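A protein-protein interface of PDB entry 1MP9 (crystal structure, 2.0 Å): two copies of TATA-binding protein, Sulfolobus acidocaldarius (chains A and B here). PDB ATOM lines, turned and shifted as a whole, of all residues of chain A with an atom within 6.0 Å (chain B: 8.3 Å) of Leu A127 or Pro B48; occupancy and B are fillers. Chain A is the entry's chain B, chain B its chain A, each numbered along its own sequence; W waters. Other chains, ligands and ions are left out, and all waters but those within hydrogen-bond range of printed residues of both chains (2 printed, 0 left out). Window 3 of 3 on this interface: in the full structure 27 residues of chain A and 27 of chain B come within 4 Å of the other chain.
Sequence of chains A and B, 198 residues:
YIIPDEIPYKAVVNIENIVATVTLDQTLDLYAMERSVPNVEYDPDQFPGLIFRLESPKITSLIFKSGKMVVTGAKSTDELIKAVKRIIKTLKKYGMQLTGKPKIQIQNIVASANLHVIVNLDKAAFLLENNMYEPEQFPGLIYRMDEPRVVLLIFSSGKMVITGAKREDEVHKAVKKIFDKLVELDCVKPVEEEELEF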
ATOM      1  N   ASP A 122      19.642  29.696 -23.801  1.00  0.00           N
ATOM      2  CA  ASP A 122      19.070  28.512 -24.426  1.00  0.00           C
ATOM      3  C   ASP A 122      18.267  27.727 -23.404  1.00  0.00           C
ATOM      4  O   ASP A 122      17.166  27.237 -23.720  1.00  0.00           O
ATOM      5  CB  ASP A 122      20.186  27.635 -24.967  1.00  0.00           C
ATOM      6  CG  ASP A 122      20.994  28.328 -26.035  1.00  0.00           C
ATOM      7  OD1 ASP A 122      20.508  28.406 -27.182  1.00  0.00           O
ATOM      8  OD2 ASP A 122      22.106  28.820 -25.730  1.00  0.00           O
ATOM      9  N   LYS A 123      18.813  27.603 -22.190  1.00  0.00           N
ATOM     10  CA  LYS A 123      18.116  26.845 -21.161  1.00  0.00           C
ATOM     11  C   LYS A 123      16.933  27.628 -20.608  1.00  0.00           C
ATOM     12  O   LYS A 123      15.866  27.063 -20.414  1.00  0.00           O
ATOM     13  CB  LYS A 123      19.067  26.466 -20.034  1.00  0.00           C
ATOM     14  CG  LYS A 123      18.467  25.598 -18.914  1.00  0.00           C
ATOM     15  CD  LYS A 123      19.565  25.299 -17.894  1.00  0.00           C
ATOM     16  CE  LYS A 123      19.162  24.233 -16.877  1.00  0.00           C
ATOM     17  NZ  LYS A 123      20.312  23.903 -15.938  1.00  0.00           N
ATOM     18  N   ALA A 124      17.123  28.920 -20.343  1.00  0.00           N
ATOM     19  CA  ALA A 124      16.024  29.733 -19.837  1.00  0.00           C
ATOM     20  C   ALA A 124      14.884  29.789 -20.857  1.00  0.00           C
ATOM     21  O   ALA A 124      13.706  29.787 -20.488  1.00  0.00           O
ATOM     22  CB  ALA A 124      16.499  31.163 -19.505  1.00  0.00           C
ATOM     23  N   ALA A 125      15.226  29.852 -22.139  1.00  0.00           N
ATOM     24  CA  ALA A 125      14.202  29.909 -23.169  1.00  0.00           C
ATOM     25  C   ALA A 125      13.157  28.776 -23.047  1.00  0.00           C
ATOM     26  O   ALA A 125      11.965  29.008 -23.226  1.00  0.00           O
ATOM     27  CB  ALA A 125      14.841  29.870 -24.538  1.00  0.00           C
ATOM     28  N   PHE A 126      13.584  27.564 -22.715  1.00  0.00           N
ATOM     29  CA  PHE A 126      12.611  26.502 -22.619  1.00  0.00           C
ATOM     30  C   PHE A 126      12.101  26.218 -21.213  1.00  0.00           C
ATOM     31  O   PHE A 126      11.226  25.382 -21.024  1.00  0.00           O
ATOM     32  CB  PHE A 126      13.156  25.238 -23.280  1.00  0.00           C
ATOM     33  CG  PHE A 126      13.422  25.410 -24.741  1.00  0.00           C
ATOM     34  CD1 PHE A 126      14.729  25.406 -25.229  1.00  0.00           C
ATOM     35  CD2 PHE A 126      12.380  25.669 -25.614  1.00  0.00           C
ATOM     36  CE1 PHE A 126      15.001  25.672 -26.589  1.00  0.00           C
ATOM     37  CE2 PHE A 126      12.629  25.938 -26.974  1.00  0.00           C
ATOM     38  CZ  PHE A 126      13.947  25.941 -27.462  1.00  0.00           C
ATOM     39  N   LEU A 127      12.623  26.914 -20.215  1.00  0.00           N
ATOM     40  CA  LEU A 127      12.137  26.677 -18.875  1.00  0.00           C
ATOM     41  C   LEU A 127      11.261  27.826 -18.352  1.00  0.00           C
ATOM     42  O   LEU A 127      10.498  27.659 -17.394  1.00  0.00           O
ATOM     43  CB  LEU A 127      13.316  26.394 -17.938  1.00  0.00           C
ATOM     44  CG  LEU A 127      14.125  25.137 -18.318  1.00  0.00           C
ATOM     45  CD1 LEU A 127      15.280  24.942 -17.339  1.00  0.00           C
ATOM     46  CD2 LEU A 127      13.211  23.911 -18.326  1.00  0.00           C
ATOM     47  N   LEU A 128      11.371  28.996 -18.965  1.00  0.00           N
ATOM     48  CA  LEU A 128      10.547  30.127 -18.549  1.00  0.00           C
ATOM     49  C   LEU A 128       9.372  30.151 -19.507  1.00  0.00           C
ATOM     50  O   LEU A 128       9.402  29.525 -20.556  1.00  0.00           O
ATOM     51  CB  LEU A 128      11.298  31.450 -18.730  1.00  0.00           C
ATOM     52  CG  LEU A 128      12.462  31.882 -17.847  1.00  0.00           C
ATOM     53  CD1 LEU A 128      13.199  33.052 -18.482  1.00  0.00           C
ATOM     54  CD2 LEU A 128      11.934  32.264 -16.500  1.00  0.00           C
ATOM     55  N   GLU A 129       8.338  30.887 -19.162  1.00  0.00           N
ATOM     56  CA  GLU A 129       7.214  31.038 -20.070  1.00  0.00           C
ATOM     57  C   GLU A 129       7.344  32.442 -20.646  1.00  0.00           C
ATOM     58  O   GLU A 129       8.322  33.136 -20.380  1.00  0.00           O
ATOM     59  CB  GLU A 129       5.900  30.950 -19.297  1.00  0.00           C
ATOM     60  CG  GLU A 129       5.438  29.529 -19.024  1.00  0.00           C
ATOM     61  CD  GLU A 129       5.075  28.803 -20.307  1.00  0.00           C
ATOM     62  OE1 GLU A 129       4.184  29.284 -21.043  1.00  0.00           O
ATOM     63  OE2 GLU A 129       5.685  27.753 -20.580  1.00  0.00           O
ATOM     64  N   ASN A 131       8.242  34.026 -23.434  1.00  0.00           N
ATOM     65  CA  ASN A 131       9.467  34.589 -23.960  1.00  0.00           C
ATOM     66  C   ASN A 131       9.819  34.201 -25.370  1.00  0.00           C
ATOM     67  O   ASN A 131       9.304  33.240 -25.940  1.00  0.00           O
ATOM     68  CB  ASN A 131      10.622  34.172 -23.057  1.00  0.00           C
ATOM     69  CG  ASN A 131      11.141  32.791 -23.404  1.00  0.00           C
ATOM     70  OD1 ASN A 131      11.896  32.633 -24.366  1.00  0.00           O
ATOM     71  ND2 ASN A 131      10.715  31.770 -22.640  1.00  0.00           N
ATOM     72  N   LEU A 185      15.579  28.026 -11.721  1.00  0.00           N
ATOM     73  CA  LEU A 185      15.644  27.144 -12.908  1.00  0.00           C
ATOM     74  C   LEU A 185      17.082  26.704 -13.221  1.00  0.00           C
ATOM     75  O   LEU A 185      17.325  25.976 -14.190  1.00  0.00           O
ATOM     76  CB  LEU A 185      15.041  27.857 -14.127  1.00  0.00           C
ATOM     77  CG  LEU A 185      13.581  28.291 -13.931  1.00  0.00           C
ATOM     78  CD1 LEU A 185      13.081  29.093 -15.170  1.00  0.00           C
ATOM     79  CD2 LEU A 185      12.723  27.030 -13.674  1.00  0.00           C
ATOM     80  N   CYS A 187      19.667  28.477 -14.291  1.00  0.00           N
ATOM     81  CA  CYS A 187      20.037  29.056 -15.583  1.00  0.00           C
ATOM     82  C   CYS A 187      21.109  30.138 -15.486  1.00  0.00           C
ATOM     83  O   CYS A 187      21.375  30.836 -16.464  1.00  0.00           O
ATOM     84  CB  CYS A 187      18.795  29.643 -16.256  1.00  0.00           C
ATOM     85  SG  CYS A 187      17.648  28.379 -16.896  1.00  0.00           S
ATOM     86  N   LEU B  28       7.102   9.355 -18.259  1.00  0.00           N
ATOM     87  CA  LEU B  28       8.148   8.716 -19.038  1.00  0.00           C
ATOM     88  C   LEU B  28       9.442   8.596 -18.264  1.00  0.00           C
ATOM     89  O   LEU B  28       9.813   9.494 -17.508  1.00  0.00           O
ATOM     90  CB  LEU B  28       8.418   9.519 -20.327  1.00  0.00           C
ATOM     91  CG  LEU B  28       7.383   9.665 -21.458  1.00  0.00           C
ATOM     92  CD1 LEU B  28       7.873  10.775 -22.412  1.00  0.00           C
ATOM     93  CD2 LEU B  28       7.196   8.360 -22.236  1.00  0.00           C
ATOM     94  N   LEU B  30      12.978   8.847 -18.699  1.00  0.00           N
ATOM     95  CA  LEU B  30      13.950   9.404 -19.650  1.00  0.00           C
ATOM     96  C   LEU B  30      15.269   8.651 -19.698  1.00  0.00           C
ATOM     97  O   LEU B  30      15.925   8.589 -20.747  1.00  0.00           O
ATOM     98  CB  LEU B  30      14.160  10.913 -19.352  1.00  0.00           C
ATOM     99  CG  LEU B  30      12.839  11.687 -19.431  1.00  0.00           C
ATOM    100  CD1 LEU B  30      13.099  13.162 -19.114  1.00  0.00           C
ATOM    101  CD2 LEU B  30      12.194  11.565 -20.829  1.00  0.00           C
ATOM    102  N   GLU B  41      19.949  12.945 -26.171  1.00  0.00           N
ATOM    103  CA  GLU B  41      20.707  13.336 -25.009  1.00  0.00           C
ATOM    104  C   GLU B  41      19.846  13.525 -23.771  1.00  0.00           C
ATOM    105  O   GLU B  41      18.758  14.128 -23.839  1.00  0.00           O
ATOM    106  CB  GLU B  41      21.449  14.624 -25.323  1.00  0.00           C
ATOM    107  CG  GLU B  41      22.420  15.041 -24.254  1.00  0.00           C
ATOM    108  CD  GLU B  41      23.365  16.114 -24.752  1.00  0.00           C
ATOM    109  OE1 GLU B  41      22.930  17.218 -25.111  1.00  0.00           O
ATOM    110  OE2 GLU B  41      24.672  15.793 -24.793  1.00  0.00           O
ATOM    111  N   TYR B  42      20.341  13.029 -22.637  1.00  0.00           N
ATOM    112  CA  TYR B  42      19.626  13.173 -21.377  1.00  0.00           C
ATOM    113  C   TYR B  42      20.588  13.232 -20.221  1.00  0.00           C
ATOM    114  O   TYR B  42      21.197  12.237 -19.866  1.00  0.00           O
ATOM    115  CB  TYR B  42      18.655  12.018 -21.142  1.00  0.00           C
ATOM    116  CG  TYR B  42      17.911  12.137 -19.827  1.00  0.00           C
ATOM    117  CD1 TYR B  42      17.195  13.300 -19.508  1.00  0.00           C
ATOM    118  CD2 TYR B  42      17.931  11.093 -18.894  1.00  0.00           C
ATOM    119  CE1 TYR B  42      16.527  13.413 -18.294  1.00  0.00           C
ATOM    120  CE2 TYR B  42      17.261  11.195 -17.669  1.00  0.00           C
ATOM    121  CZ  TYR B  42      16.567  12.353 -17.378  1.00  0.00           C
ATOM    122  OH  TYR B  42      15.927  12.463 -16.171  1.00  0.00           O
ATOM    123  N   ASP B  43      20.731  14.410 -19.637  1.00  0.00           N
ATOM    124  CA  ASP B  43      21.616  14.576 -18.495  1.00  0.00           C
ATOM    125  C   ASP B  43      20.827  15.460 -17.545  1.00  0.00           C
ATOM    126  O   ASP B  43      20.869  16.680 -17.633  1.00  0.00           O
ATOM    127  CB  ASP B  43      22.915  15.243 -18.936  1.00  0.00           C
ATOM    128  CG  ASP B  43      23.830  15.554 -17.769  1.00  0.00           C
ATOM    129  OD1 ASP B  43      23.409  15.353 -16.596  1.00  0.00           O
ATOM    130  OD2 ASP B  43      24.970  16.017 -18.038  1.00  0.00           O
ATOM    131  N   PRO B  44      20.101  14.841 -16.606  1.00  0.00           N
ATOM    132  CA  PRO B  44      19.304  15.641 -15.688  1.00  0.00           C
ATOM    133  C   PRO B  44      20.101  16.598 -14.822  1.00  0.00           C
ATOM    134  O   PRO B  44      19.522  17.469 -14.193  1.00  0.00           O
ATOM    135  CB  PRO B  44      18.497  14.584 -14.909  1.00  0.00           C
ATOM    136  CG  PRO B  44      19.466  13.413 -14.851  1.00  0.00           C
ATOM    137  CD  PRO B  44      20.113  13.410 -16.220  1.00  0.00           C
ATOM    138  N   ASP B  45      21.424  16.468 -14.792  1.00  0.00           N
ATOM    139  CA  ASP B  45      22.201  17.441 -14.009  1.00  0.00           C
ATOM    140  C   ASP B  45      22.343  18.757 -14.793  1.00  0.00           C
ATOM    141  O   ASP B  45      22.679  19.789 -14.222  1.00  0.00           O
ATOM    142  CB  ASP B  45      23.605  16.931 -13.682  1.00  0.00           C
ATOM    143  CG  ASP B  45      23.602  15.817 -12.657  1.00  0.00           C
ATOM    144  OD1 ASP B  45      22.779  15.865 -11.697  1.00  0.00           O
ATOM    145  OD2 ASP B  45      24.444  14.898 -12.809  1.00  0.00           O
ATOM    146  N   GLN B  46      22.081  18.715 -16.097  1.00  0.00           N
ATOM    147  CA  GLN B  46      22.198  19.904 -16.940  1.00  0.00           C
ATOM    148  C   GLN B  46      20.865  20.466 -17.434  1.00  0.00           C
ATOM    149  O   GLN B  46      20.699  21.674 -17.530  1.00  0.00           O
ATOM    150  CB  GLN B  46      23.069  19.596 -18.146  1.00  0.00           C
ATOM    151  CG  GLN B  46      24.551  19.512 -17.850  1.00  0.00           C
ATOM    152  CD  GLN B  46      25.355  19.366 -19.131  1.00  0.00           C
ATOM    153  OE1 GLN B  46      25.215  18.375 -19.861  1.00  0.00           O
ATOM    154  NE2 GLN B  46      26.192  20.361 -19.426  1.00  0.00           N
ATOM    155  N   PHE B  47      19.930  19.581 -17.775  1.00  0.00           N
ATOM    156  CA  PHE B  47      18.625  19.986 -18.267  1.00  0.00           C
ATOM    157  C   PHE B  47      17.644  18.871 -17.943  1.00  0.00           C
ATOM    158  O   PHE B  47      17.955  17.708 -18.160  1.00  0.00           O
ATOM    159  CB  PHE B  47      18.687  20.222 -19.772  1.00  0.00           C
ATOM    160  CG  PHE B  47      17.431  20.823 -20.333  1.00  0.00           C
ATOM    161  CD1 PHE B  47      17.107  22.149 -20.071  1.00  0.00           C
ATOM    162  CD2 PHE B  47      16.561  20.058 -21.099  1.00  0.00           C
ATOM    163  CE1 PHE B  47      15.931  22.711 -20.563  1.00  0.00           C
ATOM    164  CE2 PHE B  47      15.388  20.606 -21.596  1.00  0.00           C
ATOM    165  CZ  PHE B  47      15.074  21.942 -21.324  1.00  0.00           C
ATOM    166  N   PRO B  48      16.439  19.214 -17.434  1.00  0.00           N
ATOM    167  CA  PRO B  48      15.409  18.223 -17.060  1.00  0.00           C
ATOM    168  C   PRO B  48      14.807  17.375 -18.150  1.00  0.00           C
ATOM    169  O   PRO B  48      14.223  16.316 -17.859  1.00  0.00           O
ATOM    170  CB  PRO B  48      14.349  19.043 -16.340  1.00  0.00           C
ATOM    171  CG  PRO B  48      14.488  20.422 -16.949  1.00  0.00           C
ATOM    172  CD  PRO B  48      15.947  20.601 -17.297  1.00  0.00           C
ATOM    173  N   GLY B  49      14.954  17.804 -19.400  1.00  0.00           N
ATOM    174  CA  GLY B  49      14.375  17.028 -20.481  1.00  0.00           C
ATOM    175  C   GLY B  49      15.348  16.282 -21.361  1.00  0.00           C
ATOM    176  O   GLY B  49      16.531  16.616 -21.413  1.00  0.00           O
ATOM    177  N   LEU B  50      14.831  15.253 -22.040  1.00  0.00           N
ATOM    178  CA  LEU B  50      15.595  14.472 -22.994  1.00  0.00           C
ATOM    179  C   LEU B  50      15.528  15.300 -24.290  1.00  0.00           C
ATOM    180  O   LEU B  50      14.446  15.769 -24.701  1.00  0.00           O
ATOM    181  CB  LEU B  50      14.944  13.082 -23.229  1.00  0.00           C
ATOM    182  CG  LEU B  50      15.712  12.136 -24.158  1.00  0.00           C
ATOM    183  CD1 LEU B  50      15.512  10.683 -23.675  1.00  0.00           C
ATOM    184  CD2 LEU B  50      15.250  12.317 -25.615  1.00  0.00           C
ATOM    185  N   ILE B  51      16.677  15.458 -24.940  1.00  0.00           N
ATOM    186  CA  ILE B  51      16.771  16.252 -26.167  1.00  0.00           C
ATOM    187  C   ILE B  51      16.830  15.350 -27.387  1.00  0.00           C
ATOM    188  O   ILE B  51      17.772  14.562 -27.552  1.00  0.00           O
ATOM    189  CB  ILE B  51      18.019  17.147 -26.108  1.00  0.00           C
ATOM    190  CG1 ILE B  51      17.924  18.004 -24.854  1.00  0.00           C
ATOM    191  CG2 ILE B  51      18.146  18.002 -27.419  1.00  0.00           C
ATOM    192  CD1 ILE B  51      19.207  18.737 -24.447  1.00  0.00           C
ATOM    193  N   LEU B  62      12.118  18.524 -27.003  1.00  0.00           N
ATOM    194  CA  LEU B  62      12.562  18.366 -25.609  1.00  0.00           C
ATOM    195  C   LEU B  62      11.459  17.541 -24.962  1.00  0.00           C
ATOM    196  O   LEU B  62      10.296  17.972 -24.947  1.00  0.00           O
ATOM    197  CB  LEU B  62      12.681  19.732 -24.925  1.00  0.00           C
ATOM    198  CG  LEU B  62      13.540  20.735 -25.709  1.00  0.00           C
ATOM    199  CD1 LEU B  62      13.497  22.080 -25.042  1.00  0.00           C
ATOM    200  CD2 LEU B  62      15.001  20.233 -25.771  1.00  0.00           C
ATOM    201  N   ILE B  63      11.834  16.371 -24.428  1.00  0.00           N
ATOM    202  CA  ILE B  63      10.880  15.442 -23.841  1.00  0.00           C
ATOM    203  C   ILE B  63      11.008  15.362 -22.323  1.00  0.00           C
ATOM    204  O   ILE B  63      12.052  14.998 -21.782  1.00  0.00           O
ATOM    205  CB  ILE B  63      11.056  14.036 -24.502  1.00  0.00           C
ATOM    206  CG1 ILE B  63      10.846  14.168 -26.012  1.00  0.00           C
ATOM    207  CG2 ILE B  63      10.028  13.034 -23.968  1.00  0.00           C
ATOM    208  CD1 ILE B  63      11.241  12.921 -26.817  1.00  0.00           C
ATOM    209  N   PHE B  64       9.932  15.711 -21.637  1.00  0.00           N
ATOM    210  CA  PHE B  64       9.945  15.701 -20.182  1.00  0.00           C
ATOM    211  C   PHE B  64       9.290  14.473 -19.552  1.00  0.00           C
ATOM    212  O   PHE B  64       8.478  13.799 -20.188  1.00  0.00           O
ATOM    213  CB  PHE B  64       9.313  16.991 -19.658  1.00  0.00           C
ATOM    214  CG  PHE B  64      10.014  18.222 -20.142  1.00  0.00           C
ATOM    215  CD1 PHE B  64       9.678  18.789 -21.385  1.00  0.00           C
ATOM    216  CD2 PHE B  64      11.081  18.765 -19.412  1.00  0.00           C
ATOM    217  CE1 PHE B  64      10.409  19.889 -21.901  1.00  0.00           C
ATOM    218  CE2 PHE B  64      11.812  19.851 -19.912  1.00  0.00           C
ATOM    219  CZ  PHE B  64      11.483  20.411 -21.148  1.00  0.00           C
ATOM    220  N   LYS B  65       9.675  14.168 -18.313  1.00  0.00           N
ATOM    221  CA  LYS B  65       9.133  13.005 -17.594  1.00  0.00           C
ATOM    222  C   LYS B  65       7.610  13.016 -17.547  1.00  0.00           C
ATOM    223  O   LYS B  65       6.984  11.973 -17.521  1.00  0.00           O
ATOM    224  CB  LYS B  65       9.663  12.961 -16.159  1.00  0.00           C
ATOM    225  CG  LYS B  65      11.165  12.798 -16.080  1.00  0.00           C
ATOM    226  CD  LYS B  65      11.663  12.612 -14.646  1.00  0.00           C
ATOM    227  CE  LYS B  65      11.413  13.844 -13.797  1.00  0.00           C
ATOM    228  NZ  LYS B  65      12.074  13.718 -12.458  1.00  0.00           N
ATOM    229  N   SER B  66       7.014  14.196 -17.537  1.00  0.00           N
ATOM    230  CA  SER B  66       5.557  14.315 -17.495  1.00  0.00           C
ATOM    231  C   SER B  66       4.889  13.897 -18.790  1.00  0.00           C
ATOM    232  O   SER B  66       3.662  13.857 -18.857  1.00  0.00           O
ATOM    233  CB  SER B  66       5.177  15.757 -17.223  1.00  0.00           C
ATOM    234  OG  SER B  66       5.547  16.549 -18.347  1.00  0.00           O
ATOM    235  N   LYS B  68       5.149  15.622 -21.433  1.00  0.00           N
ATOM    236  CA  LYS B  68       4.982  16.835 -22.202  1.00  0.00           C
ATOM    237  C   LYS B  68       6.182  16.912 -23.128  1.00  0.00           C
ATOM    238  O   LYS B  68       7.318  16.673 -22.707  1.00  0.00           O
ATOM    239  CB  LYS B  68       4.992  18.075 -21.308  1.00  0.00           C
ATOM    240  CG  LYS B  68       4.789  19.358 -22.124  1.00  0.00           C
ATOM    241  CD  LYS B  68       5.436  20.586 -21.487  1.00  0.00           C
ATOM    242  CE  LYS B  68       4.801  20.991 -20.185  1.00  0.00           C
ATOM    243  NZ  LYS B  68       5.304  22.343 -19.765  1.00  0.00           N
ATOM    244  N   VAL B  70       8.151  19.463 -25.935  1.00  0.00           N
ATOM    245  CA  VAL B  70       8.204  20.790 -26.535  1.00  0.00           C
ATOM    246  C   VAL B  70       8.943  20.615 -27.861  1.00  0.00           C
ATOM    247  O   VAL B  70      10.042  20.071 -27.880  1.00  0.00           O
ATOM    248  CB  VAL B  70       8.971  21.797 -25.656  1.00  0.00           C
ATOM    249  CG1 VAL B  70       9.110  23.149 -26.435  1.00  0.00           C
ATOM    250  CG2 VAL B  70       8.202  22.045 -24.323  1.00  0.00           C
HETATM  251  O   HOH W   1      18.787  21.747 -14.732  1.00  0.00           O
HETATM  252  O   HOH W   2      22.930  23.697 -17.275  1.00  0.00           O
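Water W1 bridges NZ of Lys A123 (2.9 Å) and O of Gln B46 (3.4 Å).
Water W2 bridges the side-chain amino group (NZ) of Lys A123 and the backbone carbonyl oxygen (O) of Gln B46.
Among the printed residues, pairs that only touch across the chains: Lys A123 with Phe B47, Phe A126 with Leu B62, Leu A127 with Phe B47 and Leu A127 with Pro B48.
Of the printed residues of chain B, Leu A127 touches Phe B47 (3.7 Å) and Pro B48 (3.96 Å).
Of chain A, only Leu A127 comes within 4 Å of Pro B48.
Of the printed residues of chain B, Phe A126 touches Leu B62 (3.3 Å).
Printed residues of chain B within 4 Å of Lys A123: Gln B46 (2.8 Å) and Phe B47 (3.9 Å).
Glu B41 touches none of the printed residues of chain A.
Phe B64 touches none of the printed residues of chain A.
The nearest residue of chain A that does not touch Pro B48 is Lys A123 (4.9 Å).
No position is printed for both chains.
Of the 5 pairs that touch across the chains among the printed residues, none has its exchanged pair printed and touching as well.
The backbone carbonyl oxygen (O) of Gln B46 is in hydrogen-bond range of the side-chain amino group (NZ) of Lys A123, 2.8 Å away.
Hydrophobic or aromatic side chains of chain A within 4 Å of the printed part of chain B: Phe A126 and Leu A127.
Hydrophobic or aromatic side chains of chain B within 4 Å of the printed part of chain A: Phe B47, Pro B48 and Leu B62.
OD2 of Asp B43 sits close to OE1 of Gln B46 (3.0 Å).
The backbone carbonyl oxygen (O) of Val B70 lies within hydrogen-bond range of the backbone NH (N) of Leu B62, at 2.7 Å.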
